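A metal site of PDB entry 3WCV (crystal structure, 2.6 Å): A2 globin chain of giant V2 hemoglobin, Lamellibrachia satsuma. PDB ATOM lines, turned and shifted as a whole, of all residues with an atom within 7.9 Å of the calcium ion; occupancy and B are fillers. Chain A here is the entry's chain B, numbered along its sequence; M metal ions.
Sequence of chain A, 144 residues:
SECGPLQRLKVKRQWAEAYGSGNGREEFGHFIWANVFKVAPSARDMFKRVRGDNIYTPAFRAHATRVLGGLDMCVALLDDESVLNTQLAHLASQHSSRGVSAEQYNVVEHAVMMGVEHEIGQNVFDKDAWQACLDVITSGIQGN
Three residues have an atom within 4 Å of the calcium ion: Asn 106, Glu 109 and Asp 135.
The calcium ion is bound by OD1 of Asp 135, OD1 of Asn 106, OE2 of Glu 109 and OE1 of Glu 109.
The side-chain carboxylate (OE1) of Glu 109 lies close to the side-chain amide oxygen (OE1) of Gln 131, at 2.7 Å. The side-chain hydroxyl (OG1) of Thr 138 lies within hydrogen-bond range of the backbone carbonyl oxygen (O) of Asp 135 (3.2 Å). ND2 of Asn 106 lies within hydrogen-bond range of O of Ala 102 (2.9 Å). The side-chain carboxylate (OE2) of Glu 109 sits close to the side-chain hydroxyl (OG1) of Thr 138.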
ATOM      1  N   ALA A 102     -24.593   5.525 -25.192  1.00  0.00           N
ATOM      2  CA  ALA A 102     -23.427   5.617 -24.332  1.00  0.00           C
ATOM      3  C   ALA A 102     -22.864   7.034 -24.317  1.00  0.00           C
ATOM      4  O   ALA A 102     -22.079   7.382 -23.437  1.00  0.00           O
ATOM      5  CB  ALA A 102     -22.362   4.645 -24.809  1.00  0.00           C
ATOM      6  N   TYR A 105     -24.967   8.995 -21.716  1.00  0.00           N
ATOM      7  CA  TYR A 105     -24.518   8.586 -20.389  1.00  0.00           C
ATOM      8  C   TYR A 105     -23.266   9.377 -20.014  1.00  0.00           C
ATOM      9  O   TYR A 105     -23.123   9.812 -18.871  1.00  0.00           O
ATOM     10  CB  TYR A 105     -24.217   7.082 -20.336  1.00  0.00           C
ATOM     11  CG  TYR A 105     -25.420   6.210 -20.035  1.00  0.00           C
ATOM     12  CD1 TYR A 105     -26.045   6.264 -18.796  1.00  0.00           C
ATOM     13  CD2 TYR A 105     -25.951   5.366 -21.012  1.00  0.00           C
ATOM     14  CE1 TYR A 105     -27.177   5.494 -18.518  1.00  0.00           C
ATOM     15  CE2 TYR A 105     -27.082   4.590 -20.754  1.00  0.00           C
ATOM     16  CZ  TYR A 105     -27.695   4.654 -19.507  1.00  0.00           C
ATOM     17  OH  TYR A 105     -28.819   3.908 -19.249  1.00  0.00           O
ATOM     18  N   ASN A 106     -22.356   9.577 -20.966  1.00  0.00           N
ATOM     19  CA  ASN A 106     -21.134  10.330 -20.695  1.00  0.00           C
ATOM     20  C   ASN A 106     -21.441  11.792 -20.427  1.00  0.00           C
ATOM     21  O   ASN A 106     -20.711  12.456 -19.701  1.00  0.00           O
ATOM     22  CB  ASN A 106     -20.143  10.238 -21.851  1.00  0.00           C
ATOM     23  CG  ASN A 106     -19.606   8.849 -22.055  1.00  0.00           C
ATOM     24  OD1 ASN A 106     -19.381   8.108 -21.094  1.00  0.00           O
ATOM     25  ND2 ASN A 106     -19.387   8.474 -23.308  1.00  0.00           N
ATOM     26  N   VAL A 107     -22.493  12.307 -21.051  1.00  0.00           N
ATOM     27  CA  VAL A 107     -22.872  13.693 -20.874  1.00  0.00           C
ATOM     28  C   VAL A 107     -23.267  13.884 -19.413  1.00  0.00           C
ATOM     29  O   VAL A 107     -22.693  14.701 -18.701  1.00  0.00           O
ATOM     30  CB  VAL A 107     -24.075  14.072 -21.771  1.00  0.00           C
ATOM     31  CG1 VAL A 107     -24.619  15.439 -21.379  1.00  0.00           C
ATOM     32  CG2 VAL A 107     -23.658  14.084 -23.229  1.00  0.00           C
ATOM     33  N   GLU A 109     -22.571  12.227 -17.043  1.00  0.00           N
ATOM     34  CA  GLU A 109     -21.388  12.014 -16.224  1.00  0.00           C
ATOM     35  C   GLU A 109     -20.678  13.323 -15.914  1.00  0.00           C
ATOM     36  O   GLU A 109     -20.349  13.637 -14.767  1.00  0.00           O
ATOM     37  CB  GLU A 109     -20.415  11.067 -16.934  1.00  0.00           C
ATOM     38  CG  GLU A 109     -20.713   9.569 -16.821  1.00  0.00           C
ATOM     39  CD  GLU A 109     -19.662   8.716 -17.541  1.00  0.00           C
ATOM     40  OE1 GLU A 109     -18.473   9.093 -17.500  1.00  0.00           O
ATOM     41  OE2 GLU A 109     -20.027   7.677 -18.139  1.00  0.00           O
ATOM     42  N   HIS A 110     -20.426  14.091 -16.981  1.00  0.00           N
ATOM     43  CA  HIS A 110     -19.741  15.390 -16.848  1.00  0.00           C
ATOM     44  C   HIS A 110     -20.650  16.389 -16.123  1.00  0.00           C
ATOM     45  O   HIS A 110     -20.171  17.224 -15.345  1.00  0.00           O
ATOM     46  CB  HIS A 110     -19.375  15.907 -18.228  1.00  0.00           C
ATOM     47  CG  HIS A 110     -18.495  17.116 -18.186  1.00  0.00           C
ATOM     48  ND1 HIS A 110     -17.184  17.060 -17.759  1.00  0.00           N
ATOM     49  CD2 HIS A 110     -18.738  18.409 -18.514  1.00  0.00           C
ATOM     50  CE1 HIS A 110     -16.645  18.265 -17.840  1.00  0.00           C
ATOM     51  NE2 HIS A 110     -17.567  19.107 -18.289  1.00  0.00           N
ATOM     52  N   MET A 113     -20.333  15.601 -12.580  1.00  0.00           N
ATOM     53  CA  MET A 113     -19.018  16.012 -12.104  1.00  0.00           C
ATOM     54  C   MET A 113     -18.956  17.513 -11.873  1.00  0.00           C
ATOM     55  O   MET A 113     -18.541  17.958 -10.813  1.00  0.00           O
ATOM     56  CB  MET A 113     -17.910  15.609 -13.096  1.00  0.00           C
ATOM     57  CG  MET A 113     -17.727  14.085 -13.239  1.00  0.00           C
ATOM     58  SD  MET A 113     -16.163  13.593 -14.054  1.00  0.00           S
ATOM     59  CE  MET A 113     -16.747  13.372 -15.672  1.00  0.00           C
ATOM     60  N   GLN A 131     -14.433  10.208 -12.469  1.00  0.00           N
ATOM     61  CA  GLN A 131     -14.593   9.667 -13.809  1.00  0.00           C
ATOM     62  C   GLN A 131     -14.586   8.153 -13.758  1.00  0.00           C
ATOM     63  O   GLN A 131     -15.498   7.494 -14.246  1.00  0.00           O
ATOM     64  CB  GLN A 131     -13.466  10.191 -14.711  1.00  0.00           C
ATOM     65  CG  GLN A 131     -13.654   9.946 -16.207  1.00  0.00           C
ATOM     66  CD  GLN A 131     -14.956  10.507 -16.725  1.00  0.00           C
ATOM     67  OE1 GLN A 131     -16.021   9.884 -16.603  1.00  0.00           O
ATOM     68  NE2 GLN A 131     -14.893  11.706 -17.311  1.00  0.00           N
ATOM     69  N   ALA A 132     -13.555   7.608 -13.114  1.00  0.00           N
ATOM     70  CA  ALA A 132     -13.412   6.172 -12.971  1.00  0.00           C
ATOM     71  C   ALA A 132     -14.657   5.500 -12.381  1.00  0.00           C
ATOM     72  O   ALA A 132     -15.198   4.553 -12.962  1.00  0.00           O
ATOM     73  CB  ALA A 132     -12.190   5.856 -12.095  1.00  0.00           C
ATOM     74  N   LEU A 134     -17.688   6.773 -12.038  1.00  0.00           N
ATOM     75  CA  LEU A 134     -18.921   7.084 -12.743  1.00  0.00           C
ATOM     76  C   LEU A 134     -18.959   6.150 -13.964  1.00  0.00           C
ATOM     77  O   LEU A 134     -20.029   5.703 -14.392  1.00  0.00           O
ATOM     78  CB  LEU A 134     -18.949   8.546 -13.189  1.00  0.00           C
ATOM     79  CG  LEU A 134     -19.401   9.559 -12.142  1.00  0.00           C
ATOM     80  CD1 LEU A 134     -19.454  10.943 -12.741  1.00  0.00           C
ATOM     81  CD2 LEU A 134     -20.776   9.180 -11.646  1.00  0.00           C
ATOM     82  N   ASP A 135     -17.785   5.862 -14.529  1.00  0.00           N
ATOM     83  CA  ASP A 135     -17.692   4.951 -15.661  1.00  0.00           C
ATOM     84  C   ASP A 135     -18.278   3.636 -15.141  1.00  0.00           C
ATOM     85  O   ASP A 135     -19.183   3.065 -15.754  1.00  0.00           O
ATOM     86  CB  ASP A 135     -16.236   4.716 -16.111  1.00  0.00           C
ATOM     87  CG  ASP A 135     -15.687   5.853 -16.994  1.00  0.00           C
ATOM     88  OD1 ASP A 135     -16.480   6.521 -17.708  1.00  0.00           O
ATOM     89  OD2 ASP A 135     -14.449   6.047 -16.994  1.00  0.00           O
ATOM     90  N   VAL A 136     -17.769   3.176 -14.006  1.00  0.00           N
ATOM     91  CA  VAL A 136     -18.220   1.942 -13.385  1.00  0.00           C
ATOM     92  C   VAL A 136     -19.727   1.927 -13.166  1.00  0.00           C
ATOM     93  O   VAL A 136     -20.354   0.873 -13.235  1.00  0.00           O
ATOM     94  CB  VAL A 136     -17.545   1.708 -11.987  1.00  0.00           C
ATOM     95  CG1 VAL A 136     -18.252   0.588 -11.230  1.00  0.00           C
ATOM     96  CG2 VAL A 136     -16.081   1.342 -12.169  1.00  0.00           C
ATOM     97  N   THR A 138     -22.274   3.992 -14.868  1.00  0.00           N
ATOM     98  CA  THR A 138     -23.046   4.048 -16.100  1.00  0.00           C
ATOM     99  C   THR A 138     -22.830   2.747 -16.850  1.00  0.00           C
ATOM    100  O   THR A 138     -23.773   2.152 -17.371  1.00  0.00           O
ATOM    101  CB  THR A 138     -22.594   5.207 -17.003  1.00  0.00           C
ATOM    102  OG1 THR A 138     -21.198   5.096 -17.275  1.00  0.00           O
ATOM    103  CG2 THR A 138     -22.890   6.531 -16.326  1.00  0.00           C
ATOM    104  N   SER A 139     -21.573   2.321 -16.909  1.00  0.00           N
ATOM    105  CA  SER A 139     -21.189   1.095 -17.576  1.00  0.00           C
ATOM    106  C   SER A 139     -22.086  -0.058 -17.150  1.00  0.00           C
ATOM    107  O   SER A 139     -22.485  -0.888 -17.971  1.00  0.00           O
ATOM    108  CB  SER A 139     -19.735   0.750 -17.257  1.00  0.00           C
ATOM    109  OG  SER A 139     -19.383  -0.497 -17.790  1.00  0.00           O
ATOM    110  N   GLN A 142     -25.817   0.262 -18.385  1.00  0.00           N
ATOM    111  CA  GLN A 142     -25.974  -0.064 -19.800  1.00  0.00           C
ATOM    112  C   GLN A 142     -25.725  -1.563 -20.004  1.00  0.00           C
ATOM    113  O   GLN A 142     -25.375  -1.999 -21.095  1.00  0.00           O
ATOM    114  CB  GLN A 142     -24.944   0.702 -20.660  1.00  0.00           C
ATOM    115  CG  GLN A 142     -24.907   2.204 -20.483  1.00  0.00           C
ATOM    116  CD  GLN A 142     -23.960   2.872 -21.481  1.00  0.00           C
ATOM    117  OE1 GLN A 142     -24.257   2.975 -22.666  1.00  0.00           O
ATOM    118  NE2 GLN A 142     -22.814   3.318 -20.988  1.00  0.00           N
HETATM  119 CA    CA M   1     -18.035   7.213 -19.357  1.00  0.00          CA
